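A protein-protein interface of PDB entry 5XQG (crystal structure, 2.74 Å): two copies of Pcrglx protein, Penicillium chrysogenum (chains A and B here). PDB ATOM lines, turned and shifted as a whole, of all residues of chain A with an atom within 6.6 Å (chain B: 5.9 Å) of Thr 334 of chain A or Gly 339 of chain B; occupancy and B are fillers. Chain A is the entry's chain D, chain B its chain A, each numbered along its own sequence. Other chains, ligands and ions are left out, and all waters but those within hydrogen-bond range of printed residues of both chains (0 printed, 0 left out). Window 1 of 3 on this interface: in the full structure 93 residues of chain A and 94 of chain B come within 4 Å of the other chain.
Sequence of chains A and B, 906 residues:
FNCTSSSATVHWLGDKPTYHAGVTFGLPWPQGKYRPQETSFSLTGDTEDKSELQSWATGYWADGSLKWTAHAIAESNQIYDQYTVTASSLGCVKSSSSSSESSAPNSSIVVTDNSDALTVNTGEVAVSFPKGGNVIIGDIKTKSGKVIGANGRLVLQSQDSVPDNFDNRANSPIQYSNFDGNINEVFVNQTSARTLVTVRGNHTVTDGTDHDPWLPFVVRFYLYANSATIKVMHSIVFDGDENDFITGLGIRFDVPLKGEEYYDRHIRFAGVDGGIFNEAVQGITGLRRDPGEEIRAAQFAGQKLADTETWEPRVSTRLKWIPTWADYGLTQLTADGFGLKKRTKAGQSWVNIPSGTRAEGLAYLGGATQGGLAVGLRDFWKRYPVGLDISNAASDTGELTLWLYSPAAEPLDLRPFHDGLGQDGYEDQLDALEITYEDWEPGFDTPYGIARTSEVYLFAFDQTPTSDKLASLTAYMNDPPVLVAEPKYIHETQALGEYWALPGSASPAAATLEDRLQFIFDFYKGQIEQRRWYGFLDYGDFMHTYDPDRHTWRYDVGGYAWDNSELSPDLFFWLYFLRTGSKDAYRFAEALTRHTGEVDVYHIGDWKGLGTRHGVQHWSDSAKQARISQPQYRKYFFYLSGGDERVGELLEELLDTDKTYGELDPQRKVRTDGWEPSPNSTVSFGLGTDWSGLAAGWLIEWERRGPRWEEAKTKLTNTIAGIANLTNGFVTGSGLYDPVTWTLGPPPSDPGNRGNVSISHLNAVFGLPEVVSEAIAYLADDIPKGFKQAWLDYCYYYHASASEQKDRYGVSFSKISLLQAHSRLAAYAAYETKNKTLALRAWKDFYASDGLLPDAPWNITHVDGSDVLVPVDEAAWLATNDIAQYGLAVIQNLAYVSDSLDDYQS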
ATOM      1  N   THR A 331     -11.406  15.183   2.119  1.00  0.00           N
ATOM      2  CA  THR A 331     -11.124  14.138   3.111  1.00  0.00           C
ATOM      3  C   THR A 331      -9.837  14.460   3.893  1.00  0.00           C
ATOM      4  O   THR A 331      -8.791  14.691   3.292  1.00  0.00           O
ATOM      5  CB  THR A 331     -10.954  12.749   2.433  1.00  0.00           C
ATOM      6  OG1 THR A 331     -10.175  12.853   1.234  1.00  0.00           O
ATOM      7  CG2 THR A 331     -12.346  12.158   2.053  1.00  0.00           C
ATOM      8  N   GLN A 332      -9.943  14.498   5.229  1.00  0.00           N
ATOM      9  CA  GLN A 332      -8.847  14.819   6.132  1.00  0.00           C
ATOM     10  C   GLN A 332      -8.651  13.568   6.964  1.00  0.00           C
ATOM     11  O   GLN A 332      -9.286  13.426   7.980  1.00  0.00           O
ATOM     12  CB  GLN A 332      -9.239  16.001   6.996  1.00  0.00           C
ATOM     13  CG  GLN A 332      -8.224  16.421   8.072  1.00  0.00           C
ATOM     14  CD  GLN A 332      -7.171  17.371   7.545  1.00  0.00           C
ATOM     15  OE1 GLN A 332      -7.482  18.475   7.131  1.00  0.00           O
ATOM     16  NE2 GLN A 332      -5.932  16.931   7.522  1.00  0.00           N
ATOM     17  N   LEU A 333      -7.803  12.643   6.506  1.00  0.00           N
ATOM     18  CA  LEU A 333      -7.699  11.274   7.067  1.00  0.00           C
ATOM     19  C   LEU A 333      -6.540  11.094   8.032  1.00  0.00           C
ATOM     20  O   LEU A 333      -6.453  10.083   8.648  1.00  0.00           O
ATOM     21  CB  LEU A 333      -7.586  10.247   5.934  1.00  0.00           C
ATOM     22  CG  LEU A 333      -8.624  10.304   4.784  1.00  0.00           C
ATOM     23  CD1 LEU A 333      -8.433   9.220   3.695  1.00  0.00           C
ATOM     24  CD2 LEU A 333     -10.029  10.235   5.355  1.00  0.00           C
ATOM     25  N   THR A 334      -5.647  12.069   8.104  1.00  0.00           N
ATOM     26  CA  THR A 334      -4.645  12.206   9.165  1.00  0.00           C
ATOM     27  C   THR A 334      -4.796  13.617   9.698  1.00  0.00           C
ATOM     28  O   THR A 334      -5.494  14.424   9.104  1.00  0.00           O
ATOM     29  CB  THR A 334      -3.199  12.100   8.640  1.00  0.00           C
ATOM     30  OG1 THR A 334      -3.029  12.958   7.493  1.00  0.00           O
ATOM     31  CG2 THR A 334      -2.849  10.685   8.253  1.00  0.00           C
ATOM     32  N   ALA A 335      -4.120  13.904  10.797  1.00  0.00           N
ATOM     33  CA  ALA A 335      -3.981  15.280  11.293  1.00  0.00           C
ATOM     34  C   ALA A 335      -3.056  16.181  10.444  1.00  0.00           C
ATOM     35  O   ALA A 335      -2.973  17.378  10.662  1.00  0.00           O
ATOM     36  CB  ALA A 335      -3.467  15.252  12.731  1.00  0.00           C
ATOM     37  N   ASP A 336      -2.341  15.606   9.493  1.00  0.00           N
ATOM     38  CA  ASP A 336      -1.330  16.335   8.783  1.00  0.00           C
ATOM     39  C   ASP A 336      -1.591  16.561   7.312  1.00  0.00           C
ATOM     40  O   ASP A 336      -0.845  17.322   6.710  1.00  0.00           O
ATOM     41  CB  ASP A 336       0.001  15.621   8.965  1.00  0.00           C
ATOM     42  CG  ASP A 336       0.490  15.700  10.375  1.00  0.00           C
ATOM     43  OD1 ASP A 336       0.738  16.829  10.827  1.00  0.00           O
ATOM     44  OD2 ASP A 336       0.625  14.647  11.029  1.00  0.00           O
ATOM     45  N   GLY A 337      -2.618  15.935   6.733  1.00  0.00           N
ATOM     46  CA  GLY A 337      -2.793  15.979   5.286  1.00  0.00           C
ATOM     47  C   GLY A 337      -4.209  15.778   4.850  1.00  0.00           C
ATOM     48  O   GLY A 337      -4.884  14.960   5.414  1.00  0.00           O
ATOM     49  N   PHE A 338      -4.665  16.515   3.842  1.00  0.00           N
ATOM     50  CA  PHE A 338      -6.028  16.339   3.341  1.00  0.00           C
ATOM     51  C   PHE A 338      -6.011  16.264   1.834  1.00  0.00           C
ATOM     52  O   PHE A 338      -5.178  16.932   1.195  1.00  0.00           O
ATOM     53  CB  PHE A 338      -7.014  17.423   3.845  1.00  0.00           C
ATOM     54  CG  PHE A 338      -6.816  18.806   3.263  1.00  0.00           C
ATOM     55  CD1 PHE A 338      -5.950  19.716   3.863  1.00  0.00           C
ATOM     56  CD2 PHE A 338      -7.546  19.228   2.161  1.00  0.00           C
ATOM     57  CE1 PHE A 338      -5.781  21.008   3.360  1.00  0.00           C
ATOM     58  CE2 PHE A 338      -7.386  20.527   1.652  1.00  0.00           C
ATOM     59  CZ  PHE A 338      -6.507  21.414   2.252  1.00  0.00           C
ATOM     60  N   THR A 357      -2.175  20.680   3.815  1.00  0.00           N
ATOM     61  CA  THR A 357      -1.939  20.067   5.100  1.00  0.00           C
ATOM     62  C   THR A 357      -3.195  19.903   5.976  1.00  0.00           C
ATOM     63  O   THR A 357      -3.665  18.799   6.190  1.00  0.00           O
ATOM     64  CB  THR A 357      -0.873  20.868   5.848  1.00  0.00           C
ATOM     65  OG1 THR A 357      -1.337  22.200   6.128  1.00  0.00           O
ATOM     66  CG2 THR A 357       0.386  20.934   5.002  1.00  0.00           C
ATOM     67  N   ARG A 358      -3.719  21.028   6.453  1.00  0.00           N
ATOM     68  CA  ARG A 358      -4.736  21.095   7.502  1.00  0.00           C
ATOM     69  C   ARG A 358      -5.889  22.015   7.142  1.00  0.00           C
ATOM     70  O   ARG A 358      -5.781  23.233   7.227  1.00  0.00           O
ATOM     71  CB  ARG A 358      -4.094  21.586   8.775  1.00  0.00           C
ATOM     72  CG  ARG A 358      -3.201  20.519   9.320  1.00  0.00           C
ATOM     73  CD  ARG A 358      -2.474  20.957  10.551  1.00  0.00           C
ATOM     74  NE  ARG A 358      -1.649  19.875  11.056  1.00  0.00           N
ATOM     75  CZ  ARG A 358      -0.836  20.004  12.084  1.00  0.00           C
ATOM     76  NH1 ARG A 358      -0.736  21.173  12.687  1.00  0.00           N
ATOM     77  NH2 ARG A 358      -0.111  18.963  12.514  1.00  0.00           N
ATOM     78  N   TRP A 381      -9.503  19.286  11.651  1.00  0.00           N
ATOM     79  CA  TRP A 381      -8.339  18.441  11.402  1.00  0.00           C
ATOM     80  C   TRP A 381      -7.790  17.786  12.662  1.00  0.00           C
ATOM     81  O   TRP A 381      -7.148  16.750  12.581  1.00  0.00           O
ATOM     82  CB  TRP A 381      -7.236  19.205  10.617  1.00  0.00           C
ATOM     83  CG  TRP A 381      -6.650  20.430  11.305  1.00  0.00           C
ATOM     84  CD1 TRP A 381      -7.004  21.717  11.097  1.00  0.00           C
ATOM     85  CD2 TRP A 381      -5.616  20.453  12.269  1.00  0.00           C
ATOM     86  NE1 TRP A 381      -6.269  22.562  11.887  1.00  0.00           N
ATOM     87  CE2 TRP A 381      -5.409  21.813  12.631  1.00  0.00           C
ATOM     88  CE3 TRP A 381      -4.841  19.462  12.878  1.00  0.00           C
ATOM     89  CZ2 TRP A 381      -4.450  22.215  13.586  1.00  0.00           C
ATOM     90  CZ3 TRP A 381      -3.880  19.845  13.835  1.00  0.00           C
ATOM     91  CH2 TRP A 381      -3.703  21.225  14.192  1.00  0.00           C
ATOM     92  N   TYR A 384      -9.790  14.332  13.261  1.00  0.00           N
ATOM     93  CA  TYR A 384      -9.756  13.472  12.074  1.00  0.00           C
ATOM     94  C   TYR A 384     -10.036  12.020  12.509  1.00  0.00           C
ATOM     95  O   TYR A 384      -9.781  11.666  13.649  1.00  0.00           O
ATOM     96  CB  TYR A 384      -8.357  13.615  11.386  1.00  0.00           C
ATOM     97  CG  TYR A 384      -7.328  12.767  12.064  1.00  0.00           C
ATOM     98  CD1 TYR A 384      -6.743  13.183  13.233  1.00  0.00           C
ATOM     99  CD2 TYR A 384      -7.057  11.478  11.602  1.00  0.00           C
ATOM    100  CE1 TYR A 384      -5.865  12.380  13.924  1.00  0.00           C
ATOM    101  CE2 TYR A 384      -6.180  10.650  12.275  1.00  0.00           C
ATOM    102  CZ  TYR A 384      -5.580  11.099  13.457  1.00  0.00           C
ATOM    103  OH  TYR A 384      -4.662  10.292  14.150  1.00  0.00           O
ATOM    104  N   PRO A 385     -10.509  11.152  11.627  1.00  0.00           N
ATOM    105  CA  PRO A 385     -10.721  11.415  10.180  1.00  0.00           C
ATOM    106  C   PRO A 385     -12.082  12.001   9.933  1.00  0.00           C
ATOM    107  O   PRO A 385     -13.064  11.460  10.438  1.00  0.00           O
ATOM    108  CB  PRO A 385     -10.647  10.024   9.547  1.00  0.00           C
ATOM    109  CG  PRO A 385     -11.033   9.096  10.662  1.00  0.00           C
ATOM    110  CD  PRO A 385     -10.593   9.720  11.954  1.00  0.00           C
ATOM    111  N   GLY B 329       1.454  -0.858  10.473  1.00  0.00           N
ATOM    112  CA  GLY B 329       1.006  -0.258   9.224  1.00  0.00           C
ATOM    113  C   GLY B 329       1.273   1.216   9.137  1.00  0.00           C
ATOM    114  O   GLY B 329       0.727   1.997   9.913  1.00  0.00           O
ATOM    115  N   LEU B 330       2.136   1.593   8.201  1.00  0.00           N
ATOM    116  CA  LEU B 330       2.300   2.998   7.781  1.00  0.00           C
ATOM    117  C   LEU B 330       1.532   3.243   6.458  1.00  0.00           C
ATOM    118  O   LEU B 330       1.745   2.525   5.472  1.00  0.00           O
ATOM    119  CB  LEU B 330       3.774   3.320   7.612  1.00  0.00           C
ATOM    120  CG  LEU B 330       4.139   4.820   7.616  1.00  0.00           C
ATOM    121  CD1 LEU B 330       5.545   5.024   8.181  1.00  0.00           C
ATOM    122  CD2 LEU B 330       4.032   5.451   6.231  1.00  0.00           C
ATOM    123  N   THR B 331       0.638   4.223   6.446  1.00  0.00           N
ATOM    124  CA  THR B 331      -0.149   4.567   5.260  1.00  0.00           C
ATOM    125  C   THR B 331       0.064   6.041   4.967  1.00  0.00           C
ATOM    126  O   THR B 331      -0.104   6.871   5.850  1.00  0.00           O
ATOM    127  CB  THR B 331      -1.651   4.289   5.459  1.00  0.00           C
ATOM    128  OG1 THR B 331      -2.066   4.677   6.779  1.00  0.00           O
ATOM    129  CG2 THR B 331      -1.935   2.794   5.276  1.00  0.00           C
ATOM    130  N   GLN B 332       0.467   6.360   3.743  1.00  0.00           N
ATOM    131  CA  GLN B 332       0.686   7.730   3.312  1.00  0.00           C
ATOM    132  C   GLN B 332      -0.299   7.942   2.175  1.00  0.00           C
ATOM    133  O   GLN B 332       0.029   7.709   0.992  1.00  0.00           O
ATOM    134  CB  GLN B 332       2.138   7.888   2.854  1.00  0.00           C
ATOM    135  CG  GLN B 332       2.525   9.235   2.274  1.00  0.00           C
ATOM    136  CD  GLN B 332       3.131  10.164   3.300  1.00  0.00           C
ATOM    137  OE1 GLN B 332       4.145   9.856   3.904  1.00  0.00           O
ATOM    138  NE2 GLN B 332       2.525  11.305   3.491  1.00  0.00           N
ATOM    139  N   THR B 334      -1.991  10.822   1.485  1.00  0.00           N
ATOM    140  CA  THR B 334      -1.833  12.144   0.826  1.00  0.00           C
ATOM    141  C   THR B 334      -0.358  12.442   0.802  1.00  0.00           C
ATOM    142  O   THR B 334       0.414  11.748   1.450  1.00  0.00           O
ATOM    143  CB  THR B 334      -2.560  13.302   1.543  1.00  0.00           C
ATOM    144  OG1 THR B 334      -2.036  13.457   2.859  1.00  0.00           O
ATOM    145  CG2 THR B 334      -4.021  13.047   1.662  1.00  0.00           C
ATOM    146  N   ASP B 336       0.987  14.877   2.222  1.00  0.00           N
ATOM    147  CA  ASP B 336       1.231  15.707   3.368  1.00  0.00           C
ATOM    148  C   ASP B 336       1.122  15.080   4.743  1.00  0.00           C
ATOM    149  O   ASP B 336       1.570  15.712   5.723  1.00  0.00           O
ATOM    150  CB  ASP B 336       0.275  16.866   3.290  1.00  0.00           C
ATOM    151  CG  ASP B 336       0.725  17.846   2.284  1.00  0.00           C
ATOM    152  OD1 ASP B 336       1.883  18.292   2.441  1.00  0.00           O
ATOM    153  OD2 ASP B 336      -0.039  18.134   1.321  1.00  0.00           O
ATOM    154  N   GLY B 337       0.565  13.869   4.835  1.00  0.00           N
ATOM    155  CA  GLY B 337       0.369  13.227   6.133  1.00  0.00           C
ATOM    156  C   GLY B 337       0.388  11.732   6.044  1.00  0.00           C
ATOM    157  O   GLY B 337      -0.143  11.181   5.108  1.00  0.00           O
ATOM    158  N   PHE B 338       0.997  11.073   7.015  1.00  0.00           N
ATOM    159  CA  PHE B 338       0.944   9.600   7.076  1.00  0.00           C
ATOM    160  C   PHE B 338       0.396   9.146   8.415  1.00  0.00           C
ATOM    161  O   PHE B 338       0.582   9.827   9.414  1.00  0.00           O
ATOM    162  CB  PHE B 338       2.316   8.930   6.759  1.00  0.00           C
ATOM    163  CG  PHE B 338       3.369   9.126   7.826  1.00  0.00           C
ATOM    164  CD1 PHE B 338       3.503   8.228   8.877  1.00  0.00           C
ATOM    165  CD2 PHE B 338       4.256  10.211   7.766  1.00  0.00           C
ATOM    166  CE1 PHE B 338       4.480   8.433   9.870  1.00  0.00           C
ATOM    167  CE2 PHE B 338       5.227  10.415   8.744  1.00  0.00           C
ATOM    168  CZ  PHE B 338       5.352   9.521   9.798  1.00  0.00           C
ATOM    169  N   GLY B 339      -0.278   7.997   8.421  1.00  0.00           N
ATOM    170  CA  GLY B 339      -0.775   7.383   9.658  1.00  0.00           C
ATOM    171  C   GLY B 339       0.133   6.227   9.961  1.00  0.00           C
ATOM    172  O   GLY B 339       0.765   5.708   9.067  1.00  0.00           O
ATOM    173  N   LEU B 340       0.214   5.833  11.222  1.00  0.00           N
ATOM    174  CA  LEU B 340       1.038   4.722  11.630  1.00  0.00           C
ATOM    175  C   LEU B 340       0.323   4.018  12.746  1.00  0.00           C
ATOM    176  O   LEU B 340      -0.114   4.675  13.697  1.00  0.00           O
ATOM    177  CB  LEU B 340       2.366   5.260  12.124  1.00  0.00           C
ATOM    178  CG  LEU B 340       3.504   4.262  12.381  1.00  0.00           C
ATOM    179  CD1 LEU B 340       3.782   3.342  11.193  1.00  0.00           C
ATOM    180  CD2 LEU B 340       4.761   5.045  12.766  1.00  0.00           C
ATOM    181  N   LYS B 341       0.176   2.699  12.649  1.00  0.00           N
ATOM    182  CA  LYS B 341      -0.508   1.933  13.706  1.00  0.00           C
ATOM    183  C   LYS B 341       0.050   0.519  13.849  1.00  0.00           C
ATOM    184  O   LYS B 341       0.655  -0.011  12.916  1.00  0.00           O
ATOM    185  CB  LYS B 341      -2.002   1.892  13.465  1.00  0.00           C
ATOM    186  CG  LYS B 341      -2.366   1.424  12.089  1.00  0.00           C
ATOM    187  CD  LYS B 341      -3.861   1.349  11.853  1.00  0.00           C
ATOM    188  CE  LYS B 341      -4.122   0.516  10.584  1.00  0.00           C
ATOM    189  NZ  LYS B 341      -5.576   0.399  10.281  1.00  0.00           N
ATOM    190  N   ASN B 352      -3.040   3.266  17.706  1.00  0.00           N
ATOM    191  CA  ASN B 352      -2.455   4.357  16.930  1.00  0.00           C
ATOM    192  C   ASN B 352      -1.124   4.772  17.515  1.00  0.00           C
ATOM    193  O   ASN B 352      -0.937   4.708  18.731  1.00  0.00           O
ATOM    194  CB  ASN B 352      -3.386   5.561  16.906  1.00  0.00           C
ATOM    195  CG  ASN B 352      -2.961   6.601  15.891  1.00  0.00           C
ATOM    196  OD1 ASN B 352      -2.923   6.346  14.684  1.00  0.00           O
ATOM    197  ND2 ASN B 352      -2.641   7.771  16.368  1.00  0.00           N
ATOM    198  N   ILE B 353      -0.220   5.196  16.624  1.00  0.00           N
ATOM    199  CA  ILE B 353       1.169   5.587  16.944  1.00  0.00           C
ATOM    200  C   ILE B 353       1.413   7.032  16.503  1.00  0.00           C
ATOM    201  O   ILE B 353       0.916   7.418  15.434  1.00  0.00           O
ATOM    202  CB  ILE B 353       2.170   4.705  16.176  1.00  0.00           C
ATOM    203  CG1 ILE B 353       1.917   3.217  16.434  1.00  0.00           C
ATOM    204  CG2 ILE B 353       3.612   5.050  16.537  1.00  0.00           C
ATOM    205  CD1 ILE B 353       2.530   2.318  15.369  1.00  0.00           C
ATOM    206  N   SER B 355       2.416  10.038  14.586  1.00  0.00           N
ATOM    207  CA  SER B 355       2.785  10.019  13.173  1.00  0.00           C
ATOM    208  C   SER B 355       3.274  11.425  12.736  1.00  0.00           C
ATOM    209  O   SER B 355       3.691  12.240  13.565  1.00  0.00           O
ATOM    210  CB  SER B 355       1.591   9.489  12.356  1.00  0.00           C
ATOM    211  OG  SER B 355       0.405  10.280  12.567  1.00  0.00           O
ATOM    212  N   GLY B 356       3.285  11.683  11.439  1.00  0.00           N
ATOM    213  CA  GLY B 356       3.560  12.999  10.987  1.00  0.00           C
ATOM    214  C   GLY B 356       3.300  13.207   9.522  1.00  0.00           C
ATOM    215  O   GLY B 356       2.396  12.597   8.931  1.00  0.00           O
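O of Asp 336 of chain B sits close to O of Asp 336 of chain A, at 3.1 Å. The side-chain carboxylate (OD2) of Asp 336 of chain A sits close to the backbone carbonyl oxygen (O) of Gly 356 of chain B, at 3.4 Å.
N of Asp 336 of chain B lies close to OG1 of Thr 334 of chain B (3.4 Å). N of Gly 337 of chain A lies close to O of Thr 357 of chain A. The side-chain amide nitrogen of Gln 332 of chain B is in hydrogen-bond range of the backbone carbonyl oxygen of Thr 334 of chain B, 3.0 Å away. The backbone NH (N) of Phe 338 of chain A sits close to the backbone carbonyl oxygen (O) of Thr 357 of chain A (3.4 Å). The backbone carbonyl oxygen of Thr 357 of chain A lies within hydrogen-bond range of the side-chain amide nitrogen of Gln 332 of chain A (3.2 Å). The side-chain hydroxyl (OG1) of Thr 334 of chain B lies within hydrogen-bond range of the backbone NH (N) of Gly 337 of chain B, at 3.3 Å.
Thr 334 of chain A touches Gly 337 of chain B. Thr 334 of chain A touches Phe 338 of chain B (CG2 to C, 3.6 Å). N of Gly 339 of chain B touches CG2 of Thr 334 of chain A, at 3.7 Å. Asp 336 of chain A touches Gly 337 of chain B (CB to CA, 3.7 Å). CA of Gly 337 of chain A touches OG1 of Thr 334 of chain B, 3.6 Å away. Asp 336 of chain B touches Gly 337 of chain A. CA of Gly 337 of chain A touches N of Gly 337 of chain B (3.99 Å). Thr 334 of chain B touches Phe 338 of chain A. Thr 357 of chain A touches Asp 336 of chain B (CG2 to OD1, 3.97 Å). Asn 352 of chain B touches Tyr 384 of chain A (ND2 to OH, 3.9 Å).
Of chain B, only Gly 337, Phe 338 and Gly 339 come within 4 Å of Thr 334 of chain A. Of the printed residues of chain B, Asp 336 of chain A touches Asp 336, Gly 337 and Gly 356. Printed residues of chain A within 4 Å of Gly 356 of chain B: Asp 336 (3.4 Å). Printed residues of chain B within 4 Å of Phe 338 of chain A: Thr 334 (3.8 Å). Of the printed residues of chain B, Tyr 384 of chain A touches Asn 352. Pro 385 of chain A touches none of the printed residues of chain B. The nearest residue of chain A that does not touch Gly 339 of chain B is Leu 333 of chain A (6.4 Å).
Printed residues of chain A that touch a printed residue of chain B: Thr 334, Asp 336, Gly 337, Phe 338, Thr 357 and Tyr 384. Hydrophobic or aromatic side chains of chain A that line the printed part of chain B: Tyr 384.
Thr 334 of chain A touches Gly 337 of chain B, and with the chains exchanged Gly 337 of chain A touches Thr 334 of chain B. Thr 334 of chain A touches Phe 338 of chain B, and with the chains exchanged Phe 338 of chain A touches Thr 334 of chain B. Asp 336 of chain A touches its own counterpart, Asp 336 of chain B. Asp 336 of chain A touches Gly 337 of chain B, and with the chains exchanged Gly 337 of chain A touches Asp 336 of chain B. Positions printed for both chains: 331, 332, 334, 336, 337 and 338. Of the 12 pairs that touch across the chains among the printed residues, 8 have their exchanged pair printed and touching as well.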
